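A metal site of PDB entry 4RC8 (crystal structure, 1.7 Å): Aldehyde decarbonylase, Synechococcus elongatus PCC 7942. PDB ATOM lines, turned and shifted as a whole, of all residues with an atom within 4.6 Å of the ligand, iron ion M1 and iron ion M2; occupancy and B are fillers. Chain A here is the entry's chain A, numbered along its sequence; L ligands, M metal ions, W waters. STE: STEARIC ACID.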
ATOM      1  N   TYR A  12     -10.174 -20.179   5.299  1.00  0.00           N
ATOM      2  CA  TYR A  12      -9.150 -19.191   5.007  1.00  0.00           C
ATOM      3  C   TYR A  12      -9.661 -18.099   4.056  1.00  0.00           C
ATOM      4  O   TYR A  12      -9.247 -16.947   4.165  1.00  0.00           O
ATOM      5  CB  TYR A  12      -7.862 -19.829   4.449  1.00  0.00           C
ATOM      6  CG  TYR A  12      -6.616 -19.029   4.784  1.00  0.00           C
ATOM      7  CD1 TYR A  12      -5.989 -19.172   6.014  1.00  0.00           C
ATOM      8  CD2 TYR A  12      -6.067 -18.137   3.858  1.00  0.00           C
ATOM      9  CE1 TYR A  12      -4.844 -18.439   6.340  1.00  0.00           C
ATOM     10  CE2 TYR A  12      -4.924 -17.399   4.170  1.00  0.00           C
ATOM     11  CZ  TYR A  12      -4.317 -17.554   5.407  1.00  0.00           C
ATOM     12  OH  TYR A  12      -3.195 -16.838   5.722  1.00  0.00           O
ATOM     13  N   ILE A  15     -11.332 -15.677   6.481  1.00  0.00           N
ATOM     14  CA  ILE A  15     -10.344 -15.085   7.409  1.00  0.00           C
ATOM     15  C   ILE A  15      -9.363 -14.142   6.714  1.00  0.00           C
ATOM     16  O   ILE A  15      -9.118 -13.028   7.191  1.00  0.00           O
ATOM     17  CB  ILE A  15      -9.539 -16.174   8.180  1.00  0.00           C
ATOM     18  CG1 ILE A  15     -10.465 -17.072   8.999  1.00  0.00           C
ATOM     19  CG2 ILE A  15      -8.471 -15.543   9.079  1.00  0.00           C
ATOM     20  CD1 ILE A  15     -11.156 -16.386  10.137  1.00  0.00           C
ATOM     21  N   ASN A  16      -8.787 -14.594   5.597  1.00  0.00           N
ATOM     22  CA  ASN A  16      -7.886 -13.777   4.796  1.00  0.00           C
ATOM     23  C   ASN A  16      -8.564 -12.483   4.339  1.00  0.00           C
ATOM     24  O   ASN A  16      -7.984 -11.412   4.441  1.00  0.00           O
ATOM     25  CB  ASN A  16      -7.367 -14.602   3.595  1.00  0.00           C
ATOM     26  CG  ASN A  16      -6.323 -13.873   2.781  1.00  0.00           C
ATOM     27  OD1 ASN A  16      -6.483 -13.705   1.566  1.00  0.00           O
ATOM     28  ND2 ASN A  16      -5.249 -13.436   3.433  1.00  0.00           N
ATOM     29  N   ILE A  18     -11.095 -11.021   5.830  1.00  0.00           N
ATOM     30  CA  ILE A  18     -11.307 -10.210   7.027  1.00  0.00           C
ATOM     31  C   ILE A  18     -10.045  -9.415   7.373  1.00  0.00           C
ATOM     32  O   ILE A  18     -10.126  -8.211   7.656  1.00  0.00           O
ATOM     33  CB  ILE A  18     -11.798 -11.050   8.226  1.00  0.00           C
ATOM     34  CG1 ILE A  18     -13.288 -11.379   8.065  1.00  0.00           C
ATOM     35  CG2 ILE A  18     -11.550 -10.329   9.548  1.00  0.00           C
ATOM     36  CD1 ILE A  18     -13.775 -12.445   9.043  1.00  0.00           C
ATOM     37  N   VAL A  19      -8.889 -10.067   7.363  1.00  0.00           N
ATOM     38  CA  VAL A  19      -7.670  -9.343   7.703  1.00  0.00           C
ATOM     39  C   VAL A  19      -7.266  -8.328   6.643  1.00  0.00           C
ATOM     40  O   VAL A  19      -6.841  -7.236   6.988  1.00  0.00           O
ATOM     41  CB  VAL A  19      -6.470 -10.264   8.104  1.00  0.00           C
ATOM     42  CG1 VAL A  19      -6.827 -11.080   9.335  1.00  0.00           C
ATOM     43  CG2 VAL A  19      -6.033 -11.141   6.965  1.00  0.00           C
ATOM     44  N   GLY A  22      -9.572  -5.398   7.175  1.00  0.00           N
ATOM     45  CA  GLY A  22      -9.222  -4.716   8.417  1.00  0.00           C
ATOM     46  C   GLY A  22      -8.013  -3.815   8.275  1.00  0.00           C
ATOM     47  O   GLY A  22      -7.996  -2.699   8.799  1.00  0.00           O
ATOM     48  N   GLU A  23      -6.997  -4.295   7.564  1.00  0.00           N
ATOM     49  CA  GLU A  23      -5.790  -3.514   7.313  1.00  0.00           C
ATOM     50  C   GLU A  23      -6.094  -2.313   6.416  1.00  0.00           C
ATOM     51  O   GLU A  23      -5.569  -1.227   6.626  1.00  0.00           O
ATOM     52  CB  GLU A  23      -4.684  -4.368   6.670  1.00  0.00           C
ATOM     53  CG  GLU A  23      -4.287  -5.638   7.431  1.00  0.00           C
ATOM     54  CD  GLU A  23      -3.626  -5.376   8.777  1.00  0.00           C
ATOM     55  OE1 GLU A  23      -3.227  -4.225   9.057  1.00  0.00           O
ATOM     56  OE2 GLU A  23      -3.487  -6.343   9.564  1.00  0.00           O
ATOM     57  N   ALA A  26      -7.872   0.178   8.455  1.00  0.00           N
ATOM     58  CA  ALA A  26      -6.943   0.816   9.381  1.00  0.00           C
ATOM     59  C   ALA A  26      -6.102   1.897   8.680  1.00  0.00           C
ATOM     60  O   ALA A  26      -5.839   2.951   9.253  1.00  0.00           O
ATOM     61  CB  ALA A  26      -6.052  -0.218  10.028  1.00  0.00           C
ATOM     62  N   TYR A  30      -6.282   5.715  10.071  1.00  0.00           N
ATOM     63  CA  TYR A  30      -5.137   6.502  10.533  1.00  0.00           C
ATOM     64  C   TYR A  30      -4.906   7.730   9.664  1.00  0.00           C
ATOM     65  O   TYR A  30      -4.543   8.775  10.193  1.00  0.00           O
ATOM     66  CB  TYR A  30      -3.872   5.654  10.682  1.00  0.00           C
ATOM     67  CG  TYR A  30      -3.906   4.769  11.915  1.00  0.00           C
ATOM     68  CD1 TYR A  30      -4.086   5.314  13.187  1.00  0.00           C
ATOM     69  CD2 TYR A  30      -3.743   3.397  11.806  1.00  0.00           C
ATOM     70  CE1 TYR A  30      -4.129   4.500  14.320  1.00  0.00           C
ATOM     71  CE2 TYR A  30      -3.781   2.567  12.924  1.00  0.00           C
ATOM     72  CZ  TYR A  30      -3.965   3.132  14.173  1.00  0.00           C
ATOM     73  OH  TYR A  30      -4.012   2.314  15.289  1.00  0.00           O
ATOM     74  N   GLU A  51      -0.021   0.081   7.813  1.00  0.00           N
ATOM     75  CA  GLU A  51      -1.246  -0.673   7.523  1.00  0.00           C
ATOM     76  C   GLU A  51      -1.308  -1.098   6.056  1.00  0.00           C
ATOM     77  O   GLU A  51      -1.726  -2.215   5.746  1.00  0.00           O
ATOM     78  CB  GLU A  51      -2.499   0.116   7.912  1.00  0.00           C
ATOM     79  CG  GLU A  51      -2.519   0.571   9.367  1.00  0.00           C
ATOM     80  CD  GLU A  51      -2.675  -0.576  10.348  1.00  0.00           C
ATOM     81  OE1 GLU A  51      -2.564  -1.754   9.939  1.00  0.00           O
ATOM     82  OE2 GLU A  51      -2.935  -0.307  11.539  1.00  0.00           O
ATOM     83  N   HIS A  54       0.888  -4.064   5.767  1.00  0.00           N
ATOM     84  CA  HIS A  54       0.203  -5.244   6.318  1.00  0.00           C
ATOM     85  C   HIS A  54      -0.802  -5.813   5.332  1.00  0.00           C
ATOM     86  O   HIS A  54      -0.862  -7.036   5.143  1.00  0.00           O
ATOM     87  CB  HIS A  54      -0.550  -4.916   7.609  1.00  0.00           C
ATOM     88  CG  HIS A  54       0.298  -4.333   8.688  1.00  0.00           C
ATOM     89  ND1 HIS A  54      -0.243  -3.747   9.815  1.00  0.00           N
ATOM     90  CD2 HIS A  54       1.645  -4.245   8.824  1.00  0.00           C
ATOM     91  CE1 HIS A  54       0.744  -3.322  10.592  1.00  0.00           C
ATOM     92  NE2 HIS A  54       1.894  -3.603  10.015  1.00  0.00           N
ATOM     93  N   PHE A  58      -0.834  -9.665   3.780  1.00  0.00           N
ATOM     94  CA  PHE A  58      -1.907 -10.641   3.907  1.00  0.00           C
ATOM     95  C   PHE A  58      -2.523 -11.035   2.563  1.00  0.00           C
ATOM     96  O   PHE A  58      -3.003 -12.153   2.402  1.00  0.00           O
ATOM     97  CB  PHE A  58      -2.961 -10.167   4.915  1.00  0.00           C
ATOM     98  CG  PHE A  58      -2.474 -10.209   6.348  1.00  0.00           C
ATOM     99  CD1 PHE A  58      -1.890 -11.360   6.862  1.00  0.00           C
ATOM    100  CD2 PHE A  58      -2.588  -9.093   7.164  1.00  0.00           C
ATOM    101  CE1 PHE A  58      -1.423 -11.408   8.173  1.00  0.00           C
ATOM    102  CE2 PHE A  58      -2.126  -9.134   8.486  1.00  0.00           C
ATOM    103  CZ  PHE A  58      -1.545 -10.289   8.984  1.00  0.00           C
ATOM    104  N   CYS A  61      -0.365 -13.758   1.545  1.00  0.00           N
ATOM    105  CA  CYS A  61      -0.673 -14.979   2.292  1.00  0.00           C
ATOM    106  C   CYS A  61      -1.781 -15.791   1.613  1.00  0.00           C
ATOM    107  O   CYS A  61      -1.695 -17.020   1.534  1.00  0.00           O
ATOM    108  CB  CYS A  61      -1.080 -14.659   3.729  1.00  0.00           C
ATOM    109  SG  CYS A  61       0.262 -14.050   4.765  1.00  0.00           S
ATOM    110  N   PHE A  78     -17.088  -5.958   8.916  1.00  0.00           N
ATOM    111  CA  PHE A  78     -16.600  -4.699   9.486  1.00  0.00           C
ATOM    112  C   PHE A  78     -17.606  -3.537   9.464  1.00  0.00           C
ATOM    113  O   PHE A  78     -17.398  -2.530  10.136  1.00  0.00           O
ATOM    114  CB  PHE A  78     -15.330  -4.261   8.757  1.00  0.00           C
ATOM    115  CG  PHE A  78     -14.075  -4.877   9.307  1.00  0.00           C
ATOM    116  CD1 PHE A  78     -13.485  -4.366  10.464  1.00  0.00           C
ATOM    117  CD2 PHE A  78     -13.474  -5.956   8.668  1.00  0.00           C
ATOM    118  CE1 PHE A  78     -12.321  -4.926  10.990  1.00  0.00           C
ATOM    119  CE2 PHE A  78     -12.304  -6.513   9.187  1.00  0.00           C
ATOM    120  CZ  PHE A  78     -11.737  -6.010  10.337  1.00  0.00           C
ATOM    121  N   GLN A 101     -10.105   2.491  16.564  1.00  0.00           N
ATOM    122  CA  GLN A 101      -9.000   1.908  15.858  1.00  0.00           C
ATOM    123  C   GLN A 101      -7.778   1.519  16.712  1.00  0.00           C
ATOM    124  O   GLN A 101      -7.310   0.440  16.612  1.00  0.00           O
ATOM    125  CB  GLN A 101      -8.524   2.853  14.750  1.00  0.00           C
ATOM    126  CG  GLN A 101      -7.292   2.374  13.956  1.00  0.00           C
ATOM    127  CD  GLN A 101      -7.483   1.046  13.223  1.00  0.00           C
ATOM    128  OE1 GLN A 101      -8.429   0.858  12.548  1.00  0.00           O
ATOM    129  NE2 GLN A 101      -6.520   0.098  13.445  1.00  0.00           N
ATOM    130  N   ILE A 105      -9.697  -2.151  18.042  1.00  0.00           N
ATOM    131  CA  ILE A 105      -9.294  -2.943  16.881  1.00  0.00           C
ATOM    132  C   ILE A 105      -7.859  -3.478  17.009  1.00  0.00           C
ATOM    133  O   ILE A 105      -7.627  -4.660  16.732  1.00  0.00           O
ATOM    134  CB  ILE A 105      -9.524  -2.173  15.562  1.00  0.00           C
ATOM    135  CG1 ILE A 105     -11.026  -2.102  15.285  1.00  0.00           C
ATOM    136  CG2 ILE A 105      -8.813  -2.865  14.411  1.00  0.00           C
ATOM    137  CD1 ILE A 105     -11.400  -1.185  14.103  1.00  0.00           C
ATOM    138  N   GLU A 106      -6.910  -2.640  17.418  1.00  0.00           N
ATOM    139  CA  GLU A 106      -5.524  -3.137  17.561  1.00  0.00           C
ATOM    140  C   GLU A 106      -5.434  -4.234  18.605  1.00  0.00           C
ATOM    141  O   GLU A 106      -4.702  -5.196  18.422  1.00  0.00           O
ATOM    142  CB  GLU A 106      -4.514  -2.024  17.891  1.00  0.00           C
ATOM    143  CG  GLU A 106      -4.431  -0.858  16.899  1.00  0.00           C
ATOM    144  CD  GLU A 106      -3.777  -1.189  15.570  1.00  0.00           C
ATOM    145  OE1 GLU A 106      -3.130  -2.259  15.428  1.00  0.00           O
ATOM    146  OE2 GLU A 106      -3.893  -0.363  14.646  1.00  0.00           O
ATOM    147  N   PHE A 108      -7.826  -6.389  19.438  1.00  0.00           N
ATOM    148  CA  PHE A 108      -8.444  -7.551  18.829  1.00  0.00           C
ATOM    149  C   PHE A 108      -7.433  -8.212  17.893  1.00  0.00           C
ATOM    150  O   PHE A 108      -7.240  -9.431  17.939  1.00  0.00           O
ATOM    151  CB  PHE A 108      -9.738  -7.114  18.107  1.00  0.00           C
ATOM    152  CG  PHE A 108     -10.537  -8.233  17.492  1.00  0.00           C
ATOM    153  CD1 PHE A 108     -10.657  -9.469  18.116  1.00  0.00           C
ATOM    154  CD2 PHE A 108     -11.212  -8.024  16.288  1.00  0.00           C
ATOM    155  CE1 PHE A 108     -11.415 -10.488  17.541  1.00  0.00           C
ATOM    156  CE2 PHE A 108     -11.977  -9.031  15.712  1.00  0.00           C
ATOM    157  CZ  PHE A 108     -12.075 -10.269  16.339  1.00  0.00           C
ATOM    158  N   ALA A 109      -6.738  -7.401  17.102  1.00  0.00           N
ATOM    159  CA  ALA A 109      -5.754  -7.904  16.149  1.00  0.00           C
ATOM    160  C   ALA A 109      -4.529  -8.513  16.823  1.00  0.00           C
ATOM    161  O   ALA A 109      -4.042  -9.566  16.407  1.00  0.00           O
ATOM    162  CB  ALA A 109      -5.334  -6.793  15.201  1.00  0.00           C
ATOM    163  N   ALA A 112      -5.656 -11.892  18.248  1.00  0.00           N
ATOM    164  CA  ALA A 112      -5.897 -12.881  17.204  1.00  0.00           C
ATOM    165  C   ALA A 112      -4.631 -13.272  16.455  1.00  0.00           C
ATOM    166  O   ALA A 112      -4.393 -14.455  16.207  1.00  0.00           O
ATOM    167  CB  ALA A 112      -6.976 -12.399  16.232  1.00  0.00           C
ATOM    168  N   TYR A 113      -3.805 -12.288  16.088  1.00  0.00           N
ATOM    169  CA  TYR A 113      -2.626 -12.572  15.296  1.00  0.00           C
ATOM    170  C   TYR A 113      -1.622 -13.419  16.082  1.00  0.00           C
ATOM    171  O   TYR A 113      -0.990 -14.314  15.519  1.00  0.00           O
ATOM    172  CB  TYR A 113      -1.980 -11.295  14.775  1.00  0.00           C
ATOM    173  CG  TYR A 113      -2.752 -10.546  13.687  1.00  0.00           C
ATOM    174  CD1 TYR A 113      -4.064 -10.888  13.344  1.00  0.00           C
ATOM    175  CD2 TYR A 113      -2.163  -9.478  13.024  1.00  0.00           C
ATOM    176  CE1 TYR A 113      -4.769 -10.191  12.355  1.00  0.00           C
ATOM    177  CE2 TYR A 113      -2.853  -8.772  12.035  1.00  0.00           C
ATOM    178  CZ  TYR A 113      -4.141  -9.131  11.705  1.00  0.00           C
ATOM    179  OH  TYR A 113      -4.815  -8.411  10.735  1.00  0.00           O
ATOM    180  N   TYR A 116      -2.774 -16.942  15.946  1.00  0.00           N
ATOM    181  CA  TYR A 116      -2.526 -17.486  14.609  1.00  0.00           C
ATOM    182  C   TYR A 116      -1.083 -17.937  14.406  1.00  0.00           C
ATOM    183  O   TYR A 116      -0.843 -18.976  13.792  1.00  0.00           O
ATOM    184  CB  TYR A 116      -2.897 -16.446  13.552  1.00  0.00           C
ATOM    185  CG  TYR A 116      -2.667 -16.856  12.118  1.00  0.00           C
ATOM    186  CD1 TYR A 116      -3.234 -18.023  11.598  1.00  0.00           C
ATOM    187  CD2 TYR A 116      -1.910 -16.055  11.266  1.00  0.00           C
ATOM    188  CE1 TYR A 116      -3.032 -18.384  10.265  1.00  0.00           C
ATOM    189  CE2 TYR A 116      -1.707 -16.398   9.940  1.00  0.00           C
ATOM    190  CZ  TYR A 116      -2.277 -17.564   9.444  1.00  0.00           C
ATOM    191  OH  TYR A 116      -2.071 -17.903   8.135  1.00  0.00           O
ATOM    192  N   VAL A 131       3.892  -8.138  11.194  1.00  0.00           N
ATOM    193  CA  VAL A 131       2.695  -7.311  11.365  1.00  0.00           C
ATOM    194  C   VAL A 131       2.402  -7.022  12.839  1.00  0.00           C
ATOM    195  O   VAL A 131       2.163  -5.874  13.204  1.00  0.00           O
ATOM    196  CB  VAL A 131       1.454  -7.954  10.683  1.00  0.00           C
ATOM    197  CG1 VAL A 131       0.208  -7.156  10.989  1.00  0.00           C
ATOM    198  CG2 VAL A 131       1.660  -8.067   9.178  1.00  0.00           C
ATOM    199  N   GLU A 135       1.674  -3.643  15.343  1.00  0.00           N
ATOM    200  CA  GLU A 135       0.426  -3.478  16.092  1.00  0.00           C
ATOM    201  C   GLU A 135       0.681  -2.993  17.519  1.00  0.00           C
ATOM    202  O   GLU A 135      -0.107  -2.204  18.044  1.00  0.00           O
ATOM    203  CB  GLU A 135      -0.404  -4.755  16.105  1.00  0.00           C
ATOM    204  CG  GLU A 135      -0.910  -5.141  14.729  1.00  0.00           C
ATOM    205  CD  GLU A 135      -1.740  -6.394  14.736  1.00  0.00           C
ATOM    206  OE1 GLU A 135      -1.529  -7.265  15.626  1.00  0.00           O
ATOM    207  OE2 GLU A 135      -2.615  -6.524  13.849  1.00  0.00           O
ATOM    208  N   HIS A 138       1.047   0.660  17.334  1.00  0.00           N
ATOM    209  CA  HIS A 138      -0.233   1.327  17.070  1.00  0.00           C
ATOM    210  C   HIS A 138      -1.036   1.469  18.350  1.00  0.00           C
ATOM    211  O   HIS A 138      -1.533   2.551  18.664  1.00  0.00           O
ATOM    212  CB  HIS A 138      -1.047   0.584  16.013  1.00  0.00           C
ATOM    213  CG  HIS A 138      -0.368   0.499  14.685  1.00  0.00           C
ATOM    214  ND1 HIS A 138      -0.872  -0.239  13.632  1.00  0.00           N
ATOM    215  CD2 HIS A 138       0.804   1.025  14.239  1.00  0.00           C
ATOM    216  CE1 HIS A 138      -0.061  -0.135  12.602  1.00  0.00           C
ATOM    217  NE2 HIS A 138       0.962   0.622  12.935  1.00  0.00           N
ATOM    218  N   VAL A 175     -16.517 -14.894  13.825  1.00  0.00           N
ATOM    219  CA  VAL A 175     -15.307 -15.451  13.235  1.00  0.00           C
ATOM    220  C   VAL A 175     -14.868 -16.769  13.893  1.00  0.00           C
ATOM    221  O   VAL A 175     -14.028 -17.500  13.352  1.00  0.00           O
ATOM    222  CB  VAL A 175     -14.154 -14.385  13.253  1.00  0.00           C
ATOM    223  CG1 VAL A 175     -13.410 -14.383  14.597  1.00  0.00           C
ATOM    224  CG2 VAL A 175     -13.208 -14.602  12.096  1.00  0.00           C
ATOM    225  N   MET A 184      -7.253 -22.032  15.687  1.00  0.00           N
ATOM    226  CA  MET A 184      -7.301 -20.966  16.680  1.00  0.00           C
ATOM    227  C   MET A 184      -8.493 -21.121  17.608  1.00  0.00           C
ATOM    228  O   MET A 184      -9.647 -20.937  17.193  1.00  0.00           O
ATOM    229  CB  MET A 184      -7.381 -19.608  15.985  1.00  0.00           C
ATOM    230  CG  MET A 184      -6.220 -19.303  15.060  1.00  0.00           C
ATOM    231  SD  MET A 184      -6.578 -17.877  14.030  1.00  0.00           S
ATOM    232  CE  MET A 184      -6.817 -16.600  15.278  1.00  0.00           C
HETATM  233  C1  STE L   1      -5.108  -3.268  12.100  1.00  0.00           C
HETATM  234  O1  STE L   1      -4.843  -2.278  12.809  1.00  0.00           O
HETATM  235  O2  STE L   1      -4.264  -3.775  11.339  1.00  0.00           O
HETATM  236  C2  STE L   1      -6.497  -3.855  12.174  1.00  0.00           C
HETATM  237  C3  STE L   1      -6.594  -5.281  11.572  1.00  0.00           C
HETATM  238  C4  STE L   1      -7.921  -5.914  11.979  1.00  0.00           C
HETATM  239  C5  STE L   1      -7.932  -7.403  11.668  1.00  0.00           C
HETATM  240  C6  STE L   1      -8.850  -8.164  12.632  1.00  0.00           C
HETATM  241  C7  STE L   1      -8.818  -9.667  12.324  1.00  0.00           C
HETATM  242  C8  STE L   1      -9.853 -10.441  13.141  1.00  0.00           C
HETATM  243  C9  STE L   1     -10.072 -11.846  12.583  1.00  0.00           C
HETATM  244  C10 STE L   1      -9.468 -12.923  13.570  1.00  0.00           C
HETATM  245  C11 STE L   1      -8.759 -14.041  12.713  1.00  0.00           C
HETATM  246  C12 STE L   1      -7.404 -13.499  12.203  1.00  0.00           C
HETATM  247  C13 STE L   1      -6.351 -14.611  12.175  1.00  0.00           C
HETATM  248  C14 STE L   1      -5.060 -14.112  11.536  1.00  0.00           C
HETATM  249  C15 STE L   1      -4.960 -14.583  10.084  1.00  0.00           C
HETATM  250  C16 STE L   1      -4.086 -13.553   9.234  1.00  0.00           C
HETATM  251  C17 STE L   1      -3.628 -14.454   7.959  1.00  0.00           C
HETATM  252  C18 STE L   1      -4.472 -14.141   6.648  1.00  0.00           C
HETATM  253 FE    FE M   1      -2.278  -3.564  10.751  1.00  0.00          FE
HETATM  254 FE    FE M   2      -2.725  -1.453  13.221  1.00  0.00          FE
HETATM  255  O   HOH W   1      -1.758  -2.850  12.332  1.00  0.00           O
HETATM  256  O   HOH W   2      -2.204  -5.376  11.453  1.00  0.00           O
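OH of Tyr 12 lies within hydrogen-bond range of OH of Tyr 116, at 2.9 Å.
O of Gln 101 lies close to N of Glu 106 (3.2 Å).
The side-chain carboxylate of Glu 23 sits at hydrogen-bond distance from the side-chain hydroxyl of Tyr 113 (2.7 Å).
The side-chain carboxylate (OE2) of Glu 106 lies close to the side-chain hydroxyl (OH) of Tyr 30, at 2.8 Å.
The side-chain amide nitrogen (ND2) of Asn 16 sits at hydrogen-bond distance from the backbone carbonyl oxygen (O) of Phe 58 (2.8 Å).
Residues that only touch the ligand: Tyr 12 (3.1 Å), Ile 105 (3.4 Å), Tyr 116 (3.4 Å), Asn 16 (3.4 Å), Val 19 (3.4 Å), Tyr 113 (3.4 Å), Phe 58 (3.6 Å), Phe 108 (3.6 Å), Ala 26 (3.7 Å), Ala 112 (3.7 Å), Ile 18 (3.7 Å), Met 184 (3.7 Å), Ile 15 (3.8 Å) and Gly 22 (3.9 Å).
Hydrophobic or aromatic side chains within 4 Å of the ligand: Tyr 12, Ile 15, Ile 18, Val 19, Ala 26, Phe 58, Ile 105, Phe 108, Ala 112, Tyr 113, Tyr 116 and Met 184.
Of the 27 residues printed, 18 come within 4 Å of the ligand.
The nearest printed residue that does not touch the ligand is Glu 135 (4.1 Å).
The side-chain amide nitrogen (NE2) of Gln 101 sits close to an oxygen (O1) of the ligand, 3.0 Å away.
Water W2 lies within hydrogen-bond range of OE2 of Glu 23 and OE2 of Glu 135.
Of the 27 residues printed, 3 come within 4 Å of iron ion M1.
Along chain A the residues within 4 Å of iron ion M1 span positions 23 to 54.
The nearest printed residue that does not touch iron ion M1 is Glu 135 (4.3 Å).
Iron ion M1 is bound by water W1 (1.8 Å), water W2 (1.9 Å), the side-chain carboxylate of Glu 51 (2.0 Å), the side-chain carboxylate of Glu 23 (2.1 Å), an oxygen (O2) of the ligand (2.1 Å) and a ring nitrogen (ND1) of His 54 (2.2 Å).
Iron ion M2 is bound by water W1 (1.9 Å), OE2 of Glu 51 (2.0 Å), OE2 of Glu 106 (2.1 Å), ND1 of His 138 (2.3 Å), O1 of the ligand (2.3 Å) and OE1 of Glu 106 (2.4 Å).
Iron ion M2 has six donor atoms within binding distance.
Within 4 Å of iron ion M2: Glu 51, Glu 106 and His 138.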
